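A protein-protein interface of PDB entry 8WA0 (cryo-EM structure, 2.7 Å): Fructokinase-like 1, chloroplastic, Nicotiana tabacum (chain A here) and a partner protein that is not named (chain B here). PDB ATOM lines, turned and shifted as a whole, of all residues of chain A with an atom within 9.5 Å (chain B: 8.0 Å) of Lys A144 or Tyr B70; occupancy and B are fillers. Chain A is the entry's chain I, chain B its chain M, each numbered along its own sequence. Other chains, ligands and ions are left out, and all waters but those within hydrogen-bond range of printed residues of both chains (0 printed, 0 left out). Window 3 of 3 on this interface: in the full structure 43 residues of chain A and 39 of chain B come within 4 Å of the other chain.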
ATOM      1  N   GLN A 139      29.150  25.279  13.083  1.00  0.00           N
ATOM      2  CA  GLN A 139      29.525  24.275  12.110  1.00  0.00           C
ATOM      3  C   GLN A 139      28.488  23.171  12.094  1.00  0.00           C
ATOM      4  O   GLN A 139      27.798  22.985  13.079  1.00  0.00           O
ATOM      5  CB  GLN A 139      30.908  23.761  12.449  1.00  0.00           C
ATOM      6  CG  GLN A 139      31.556  22.909  11.388  1.00  0.00           C
ATOM      7  CD  GLN A 139      32.871  22.385  11.881  1.00  0.00           C
ATOM      8  OE1 GLN A 139      33.401  21.399  11.372  1.00  0.00           O
ATOM      9  NE2 GLN A 139      33.398  23.036  12.907  1.00  0.00           N
ATOM     10  N   MET A 140      28.348  22.449  11.006  1.00  0.00           N
ATOM     11  CA  MET A 140      27.347  21.417  10.854  1.00  0.00           C
ATOM     12  C   MET A 140      28.052  20.079  10.699  1.00  0.00           C
ATOM     13  O   MET A 140      29.264  20.027  10.856  1.00  0.00           O
ATOM     14  CB  MET A 140      26.424  21.717   9.694  1.00  0.00           C
ATOM     15  CG  MET A 140      25.696  23.039   9.748  1.00  0.00           C
ATOM     16  SD  MET A 140      24.060  22.871  10.451  1.00  0.00           S
ATOM     17  CE  MET A 140      23.618  24.564  10.788  1.00  0.00           C
ATOM     18  N   HIS A 141      27.352  19.001  10.421  1.00  0.00           N
ATOM     19  CA  HIS A 141      27.957  17.680  10.327  1.00  0.00           C
ATOM     20  C   HIS A 141      29.009  17.560   9.271  1.00  0.00           C
ATOM     21  O   HIS A 141      28.892  18.142   8.223  1.00  0.00           O
ATOM     22  CB  HIS A 141      26.889  16.629  10.109  1.00  0.00           C
ATOM     23  CG  HIS A 141      27.282  15.233  10.443  1.00  0.00           C
ATOM     24  ND1 HIS A 141      27.738  14.346   9.499  1.00  0.00           N
ATOM     25  CD2 HIS A 141      27.213  14.544  11.601  1.00  0.00           C
ATOM     26  CE1 HIS A 141      27.983  13.185  10.071  1.00  0.00           C
ATOM     27  NE2 HIS A 141      27.669  13.278  11.346  1.00  0.00           N
ATOM     28  N   GLN A 142      30.054  16.809   9.541  1.00  0.00           N
ATOM     29  CA  GLN A 142      31.156  16.641   8.649  1.00  0.00           C
ATOM     30  C   GLN A 142      30.797  15.999   7.385  1.00  0.00           C
ATOM     31  O   GLN A 142      31.300  16.379   6.349  1.00  0.00           O
ATOM     32  CB  GLN A 142      32.191  15.791   9.330  1.00  0.00           C
ATOM     33  N   ASP A 143      29.938  15.010   7.433  1.00  0.00           N
ATOM     34  CA  ASP A 143      29.551  14.276   6.275  1.00  0.00           C
ATOM     35  C   ASP A 143      28.217  14.523   5.600  1.00  0.00           C
ATOM     36  O   ASP A 143      28.166  14.440   4.395  1.00  0.00           O
ATOM     37  CB  ASP A 143      29.631  12.833   6.676  1.00  0.00           C
ATOM     38  CG  ASP A 143      31.000  12.416   7.105  1.00  0.00           C
ATOM     39  OD1 ASP A 143      31.915  12.426   6.265  1.00  0.00           O
ATOM     40  OD2 ASP A 143      31.157  12.041   8.280  1.00  0.00           O
ATOM     41  N   LYS A 144      27.152  14.845   6.297  1.00  0.00           N
ATOM     42  CA  LYS A 144      25.830  15.001   5.742  1.00  0.00           C
ATOM     43  C   LYS A 144      25.608  16.352   5.177  1.00  0.00           C
ATOM     44  O   LYS A 144      25.406  17.282   5.911  1.00  0.00           O
ATOM     45  CB  LYS A 144      24.822  14.689   6.799  1.00  0.00           C
ATOM     46  CG  LYS A 144      24.898  13.324   7.428  1.00  0.00           C
ATOM     47  CD  LYS A 144      23.744  13.156   8.395  1.00  0.00           C
ATOM     48  CE  LYS A 144      23.835  11.845   9.147  1.00  0.00           C
ATOM     49  NZ  LYS A 144      22.720  11.704  10.122  1.00  0.00           N
ATOM     50  N   TYR A 145      25.533  16.462   3.882  1.00  0.00           N
ATOM     51  CA  TYR A 145      25.486  17.717   3.188  1.00  0.00           C
ATOM     52  C   TYR A 145      24.133  18.192   2.920  1.00  0.00           C
ATOM     53  O   TYR A 145      23.941  19.149   2.204  1.00  0.00           O
ATOM     54  CB  TYR A 145      26.327  17.633   1.922  1.00  0.00           C
ATOM     55  CG  TYR A 145      26.255  16.373   1.111  1.00  0.00           C
ATOM     56  CD1 TYR A 145      25.147  16.075   0.350  1.00  0.00           C
ATOM     57  CD2 TYR A 145      27.315  15.503   1.069  1.00  0.00           C
ATOM     58  CE1 TYR A 145      25.082  14.928  -0.398  1.00  0.00           C
ATOM     59  CE2 TYR A 145      27.260  14.352   0.322  1.00  0.00           C
ATOM     60  CZ  TYR A 145      26.137  14.074  -0.408  1.00  0.00           C
ATOM     61  OH  TYR A 145      26.070  12.936  -1.160  1.00  0.00           O
ATOM     62  N   SER A 146      23.169  17.521   3.477  1.00  0.00           N
ATOM     63  CA  SER A 146      21.838  17.881   3.332  1.00  0.00           C
ATOM     64  C   SER A 146      21.526  18.817   4.432  1.00  0.00           C
ATOM     65  O   SER A 146      20.441  19.360   4.481  1.00  0.00           O
ATOM     66  CB  SER A 146      21.075  16.627   3.492  1.00  0.00           C
ATOM     67  OG  SER A 146      21.587  15.860   4.553  1.00  0.00           O
ATOM     68  N   GLU A 147      22.482  19.042   5.310  1.00  0.00           N
ATOM     69  CA  GLU A 147      22.245  19.882   6.445  1.00  0.00           C
ATOM     70  C   GLU A 147      22.940  21.172   6.251  1.00  0.00           C
ATOM     71  O   GLU A 147      22.705  22.112   6.974  1.00  0.00           O
ATOM     72  CB  GLU A 147      22.811  19.223   7.678  1.00  0.00           C
ATOM     73  CG  GLU A 147      22.087  17.979   8.123  1.00  0.00           C
ATOM     74  CD  GLU A 147      22.588  17.498   9.462  1.00  0.00           C
ATOM     75  OE1 GLU A 147      23.539  18.113   9.984  1.00  0.00           O
ATOM     76  OE2 GLU A 147      22.032  16.515   9.991  1.00  0.00           O
ATOM     77  N   TRP A 148      23.803  21.249   5.268  1.00  0.00           N
ATOM     78  CA  TRP A 148      24.596  22.438   5.103  1.00  0.00           C
ATOM     79  C   TRP A 148      23.812  23.612   4.590  1.00  0.00           C
ATOM     80  O   TRP A 148      24.273  24.727   4.659  1.00  0.00           O
ATOM     81  CB  TRP A 148      25.814  22.150   4.252  1.00  0.00           C
ATOM     82  CG  TRP A 148      26.731  21.108   4.795  1.00  0.00           C
ATOM     83  CD1 TRP A 148      26.619  20.447   5.975  1.00  0.00           C
ATOM     84  CD2 TRP A 148      27.911  20.607   4.168  1.00  0.00           C
ATOM     85  NE1 TRP A 148      27.647  19.559   6.120  1.00  0.00           N
ATOM     86  CE2 TRP A 148      28.458  19.641   5.022  1.00  0.00           C
ATOM     87  CE3 TRP A 148      28.558  20.883   2.965  1.00  0.00           C
ATOM     88  CZ2 TRP A 148      29.617  18.949   4.714  1.00  0.00           C
ATOM     89  CZ3 TRP A 148      29.706  20.198   2.663  1.00  0.00           C
ATOM     90  CH2 TRP A 148      30.226  19.242   3.532  1.00  0.00           C
ATOM     91  N   LYS A 149      22.624  23.374   4.076  1.00  0.00           N
ATOM     92  CA  LYS A 149      21.769  24.438   3.580  1.00  0.00           C
ATOM     93  C   LYS A 149      21.358  25.366   4.669  1.00  0.00           C
ATOM     94  O   LYS A 149      21.043  26.504   4.419  1.00  0.00           O
ATOM     95  CB  LYS A 149      20.531  23.877   2.901  1.00  0.00           C
ATOM     96  CG  LYS A 149      19.694  22.932   3.738  1.00  0.00           C
ATOM     97  CD  LYS A 149      18.390  22.615   3.034  1.00  0.00           C
ATOM     98  CE  LYS A 149      18.624  21.852   1.747  1.00  0.00           C
ATOM     99  NZ  LYS A 149      19.004  20.440   2.005  1.00  0.00           N
ATOM    100  N   MET A 150      21.314  24.881   5.887  1.00  0.00           N
ATOM    101  CA  MET A 150      20.890  25.687   6.992  1.00  0.00           C
ATOM    102  C   MET A 150      21.810  26.852   7.176  1.00  0.00           C
ATOM    103  O   MET A 150      21.382  27.912   7.569  1.00  0.00           O
ATOM    104  CB  MET A 150      20.801  24.830   8.224  1.00  0.00           C
ATOM    105  CG  MET A 150      19.890  23.634   8.051  1.00  0.00           C
ATOM    106  SD  MET A 150      19.621  22.748   9.587  1.00  0.00           S
ATOM    107  CE  MET A 150      18.749  23.991  10.526  1.00  0.00           C
ATOM    108  N   ARG B  67      26.633  -1.112   6.060  1.00  0.00           N
ATOM    109  CA  ARG B  67      27.784  -0.480   5.509  1.00  0.00           C
ATOM    110  C   ARG B  67      27.660   1.002   5.587  1.00  0.00           C
ATOM    111  O   ARG B  67      26.604   1.551   5.335  1.00  0.00           O
ATOM    112  CB  ARG B  67      27.940  -0.939   4.082  1.00  0.00           C
ATOM    113  CG  ARG B  67      29.003  -0.267   3.239  1.00  0.00           C
ATOM    114  CD  ARG B  67      30.385  -0.781   3.565  1.00  0.00           C
ATOM    115  NE  ARG B  67      31.356  -0.303   2.595  1.00  0.00           N
ATOM    116  CZ  ARG B  67      32.666  -0.453   2.720  1.00  0.00           C
ATOM    117  NH1 ARG B  67      33.162  -1.061   3.786  1.00  0.00           N
ATOM    118  NH2 ARG B  67      33.480   0.015   1.786  1.00  0.00           N
ATOM    119  N   GLU B  68      28.732   1.671   5.939  1.00  0.00           N
ATOM    120  CA  GLU B  68      28.746   3.101   6.020  1.00  0.00           C
ATOM    121  C   GLU B  68      28.528   3.820   4.739  1.00  0.00           C
ATOM    122  O   GLU B  68      29.062   3.456   3.714  1.00  0.00           O
ATOM    123  CB  GLU B  68      30.082   3.507   6.547  1.00  0.00           C
ATOM    124  CG  GLU B  68      30.452   2.875   7.878  1.00  0.00           C
ATOM    125  CD  GLU B  68      31.324   1.641   7.726  1.00  0.00           C
ATOM    126  OE1 GLU B  68      31.700   1.308   6.581  1.00  0.00           O
ATOM    127  OE2 GLU B  68      31.635   1.004   8.754  1.00  0.00           O
ATOM    128  N   ASP B  69      27.733   4.849   4.783  1.00  0.00           N
ATOM    129  CA  ASP B  69      27.439   5.637   3.635  1.00  0.00           C
ATOM    130  C   ASP B  69      28.531   6.468   3.100  1.00  0.00           C
ATOM    131  O   ASP B  69      28.640   6.615   1.905  1.00  0.00           O
ATOM    132  CB  ASP B  69      26.235   6.478   3.941  1.00  0.00           C
ATOM    133  CG  ASP B  69      25.086   5.685   4.517  1.00  0.00           C
ATOM    134  OD1 ASP B  69      25.058   4.448   4.365  1.00  0.00           O
ATOM    135  OD2 ASP B  69      24.191   6.306   5.120  1.00  0.00           O
ATOM    136  N   TYR B  70      29.360   7.036   3.960  1.00  0.00           N
ATOM    137  CA  TYR B  70      30.343   7.977   3.519  1.00  0.00           C
ATOM    138  C   TYR B  70      31.700   7.383   3.573  1.00  0.00           C
ATOM    139  O   TYR B  70      32.085   6.837   4.580  1.00  0.00           O
ATOM    140  CB  TYR B  70      30.184   9.254   4.329  1.00  0.00           C
ATOM    141  CG  TYR B  70      28.831   9.922   4.254  1.00  0.00           C
ATOM    142  CD1 TYR B  70      28.564  10.852   3.290  1.00  0.00           C
ATOM    143  CD2 TYR B  70      27.844   9.653   5.171  1.00  0.00           C
ATOM    144  CE1 TYR B  70      27.346  11.465   3.194  1.00  0.00           C
ATOM    145  CE2 TYR B  70      26.620  10.270   5.095  1.00  0.00           C
ATOM    146  CZ  TYR B  70      26.380  11.174   4.104  1.00  0.00           C
ATOM    147  OH  TYR B  70      25.165  11.802   4.016  1.00  0.00           O
ATOM    148  N   LEU B  71      32.431   7.456   2.487  1.00  0.00           N
ATOM    149  CA  LEU B  71      33.721   6.828   2.376  1.00  0.00           C
ATOM    150  C   LEU B  71      34.946   7.691   2.366  1.00  0.00           C
ATOM    151  O   LEU B  71      36.020   7.175   2.138  1.00  0.00           O
ATOM    152  CB  LEU B  71      33.743   6.018   1.089  1.00  0.00           C
ATOM    153  CG  LEU B  71      33.065   4.665   0.863  1.00  0.00           C
ATOM    154  CD1 LEU B  71      31.561   4.669   1.088  1.00  0.00           C
ATOM    155  CD2 LEU B  71      33.366   4.210  -0.547  1.00  0.00           C
ATOM    156  N   VAL B  72      34.823   8.992   2.589  1.00  0.00           N
ATOM    157  CA  VAL B  72      35.947   9.905   2.641  1.00  0.00           C
ATOM    158  C   VAL B  72      36.052  10.362   4.069  1.00  0.00           C
ATOM    159  O   VAL B  72      35.052  10.717   4.645  1.00  0.00           O
ATOM    160  CB  VAL B  72      35.785  10.998   1.624  1.00  0.00           C
ATOM    161  CG1 VAL B  72      36.790  12.110   1.770  1.00  0.00           C
ATOM    162  CG2 VAL B  72      35.627  10.437   0.232  1.00  0.00           C
ATOM    163  N   LYS B  73      37.232  10.350   4.674  1.00  0.00           N
ATOM    164  CA  LYS B  73      37.380  10.624   6.090  1.00  0.00           C
ATOM    165  C   LYS B  73      38.110  11.881   6.502  1.00  0.00           C
ATOM    166  O   LYS B  73      39.051  12.265   5.853  1.00  0.00           O
ATOM    167  CB  LYS B  73      38.048   9.425   6.721  1.00  0.00           C
ATOM    168  CG  LYS B  73      37.425   8.075   6.437  1.00  0.00           C
ATOM    169  CD  LYS B  73      36.096   7.902   7.143  1.00  0.00           C
ATOM    170  CE  LYS B  73      35.450   6.586   6.752  1.00  0.00           C
ATOM    171  NZ  LYS B  73      34.086   6.442   7.332  1.00  0.00           N
ATOM    172  N   THR B  99      31.759  23.844   5.905  1.00  0.00           N
ATOM    173  CA  THR B  99      30.345  23.578   5.844  1.00  0.00           C
ATOM    174  C   THR B  99      29.622  24.753   5.241  1.00  0.00           C
ATOM    175  O   THR B  99      28.643  24.585   4.546  1.00  0.00           O
ATOM    176  CB  THR B  99      29.771  23.203   7.203  1.00  0.00           C
ATOM    177  OG1 THR B  99      30.145  24.192   8.163  1.00  0.00           O
ATOM    178  CG2 THR B  99      30.311  21.864   7.639  1.00  0.00           C
ATOM    179  N   ILE B 105      29.280  21.893  -1.363  1.00  0.00           N
ATOM    180  CA  ILE B 105      28.265  20.856  -1.392  1.00  0.00           C
ATOM    181  C   ILE B 105      28.336  20.051  -2.671  1.00  0.00           C
ATOM    182  O   ILE B 105      28.063  18.866  -2.663  1.00  0.00           O
ATOM    183  CB  ILE B 105      26.854  21.430  -1.206  1.00  0.00           C
ATOM    184  CG1 ILE B 105      26.823  22.359   0.002  1.00  0.00           C
ATOM    185  CG2 ILE B 105      25.827  20.327  -1.030  1.00  0.00           C
ATOM    186  CD1 ILE B 105      25.447  22.886   0.326  1.00  0.00           C
ATOM    187  N   ALA B 108      31.695  17.541  -2.751  1.00  0.00           N
ATOM    188  CA  ALA B 108      31.592  16.381  -1.942  1.00  0.00           C
ATOM    189  C   ALA B 108      30.996  15.229  -2.647  1.00  0.00           C
ATOM    190  O   ALA B 108      31.465  14.117  -2.499  1.00  0.00           O
ATOM    191  CB  ALA B 108      30.821  16.714  -0.736  1.00  0.00           C
ATOM    192  N   GLU B 112      33.229  11.620  -3.477  1.00  0.00           N
ATOM    193  CA  GLU B 112      32.728  10.322  -3.117  1.00  0.00           C
ATOM    194  C   GLU B 112      32.656   9.372  -4.293  1.00  0.00           C
ATOM    195  O   GLU B 112      32.900   8.191  -4.108  1.00  0.00           O
ATOM    196  CB  GLU B 112      31.493  10.360  -2.275  1.00  0.00           C
ATOM    197  CG  GLU B 112      31.737  10.551  -0.796  1.00  0.00           C
ATOM    198  CD  GLU B 112      30.465  10.486   0.011  1.00  0.00           C
ATOM    199  OE1 GLU B 112      29.966  11.557   0.417  1.00  0.00           O
ATOM    200  OE2 GLU B 112      29.955   9.368   0.235  1.00  0.00           O
ATOM    201  N   ALA B 115      36.141   7.907  -5.209  1.00  0.00           N
ATOM    202  CA  ALA B 115      36.458   6.870  -4.283  1.00  0.00           C
ATOM    203  C   ALA B 115      35.941   5.520  -4.612  1.00  0.00           C
ATOM    204  O   ALA B 115      36.643   4.550  -4.438  1.00  0.00           O
ATOM    205  CB  ALA B 115      35.972   7.273  -2.950  1.00  0.00           C
ATOM    206  N   LYS B 126      39.921  14.356   3.723  1.00  0.00           N
ATOM    207  CA  LYS B 126      39.400  15.713   3.868  1.00  0.00           C
ATOM    208  C   LYS B 126      39.770  16.544   5.102  1.00  0.00           C
ATOM    209  O   LYS B 126      39.842  16.002   6.160  1.00  0.00           O
ATOM    210  CB  LYS B 126      37.898  15.713   3.631  1.00  0.00           C
ATOM    211  CG  LYS B 126      37.054  14.952   4.615  1.00  0.00           C
ATOM    212  CD  LYS B 126      35.595  15.156   4.287  1.00  0.00           C
ATOM    213  CE  LYS B 126      34.702  14.338   5.188  1.00  0.00           C
ATOM    214  NZ  LYS B 126      33.287  14.469   4.772  1.00  0.00           N
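N of Asp A143 sits at hydrogen-bond distance from ND1 of His A141 (3.1 Å). ND1 of His A141 sits at hydrogen-bond distance from N of Lys A144 (3.3 Å). NE1 of Trp A148 is in hydrogen-bond range of O of His A141, at 2.8 Å. The indole nitrogen (NE1) of Trp A148 sits at hydrogen-bond distance from the backbone carbonyl oxygen (O) of Lys A144 (3.2 Å). The side-chain amino group (NZ) of Lys B73 lies within hydrogen-bond range of the backbone carbonyl oxygen (O) of Tyr B70, at 3.4 Å. O of Lys B73 lies within hydrogen-bond range of N of Lys B126 (3.1 Å).
The backbone carbonyl oxygen (O) of Gln A142 sits at hydrogen-bond distance from the side-chain amino group (NZ) of Lys B126, 3.2 Å away. OD1 of Asp A143 lies within salt-bridge range of NZ of Lys B126, at 2.9 Å.
Of the 12 printed residues of chain A, 7 touch a printed residue of chain B. Hydrophobic or aromatic side chains of chain A within 4 Å of the printed part of chain B: Tyr A145 and Trp A148. Of the 13 printed residues of chain B, 6 touch a printed residue of chain A. Among the printed residues, 11 pairs touch across the chains. Among the printed residues, Asp or Glu carboxylates within 4 Å of a Lys or Arg side-chain nitrogen of the other chain: Asp A143 with Lys B126.
Thr B99 touches Gln A139 (OG1 to CG, 3.7 Å). Thr B99 touches Met A140 (OG1 to N, 3.8 Å). O of Asp A143 touches CE1 of Tyr B70, 3.3 Å away. OD1 of Asp A143 touches O of Val B72 (3.9 Å). CA of Lys A144 touches OH of Tyr B70, 3.7 Å away. CG2 of Ile B105 touches O of Tyr A145, at 3.9 Å. Tyr A145 touches Glu B112 (CE2 to OE1, 3.9 Å). Trp A148 touches Thr B99. CG1 of Ile B105 touches CE3 of Trp A148, 3.7 Å away.
Of chain B, only Tyr B70 comes within 4 Å of Lys A144. Tyr B70 touches two residues of chain A. Of the printed residues of chain B, Asp A143 touches Tyr B70, Val B72 and Lys B126. Of the printed residues of chain B, Met A140 touches Thr B99 (3.8 Å). Ser A146 touches none of the printed residues of chain B. Lys B73 touches none of the printed residues of chain A. The nearest residue of chain A that does not touch Tyr B70 is Tyr A145 (4.1 Å).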
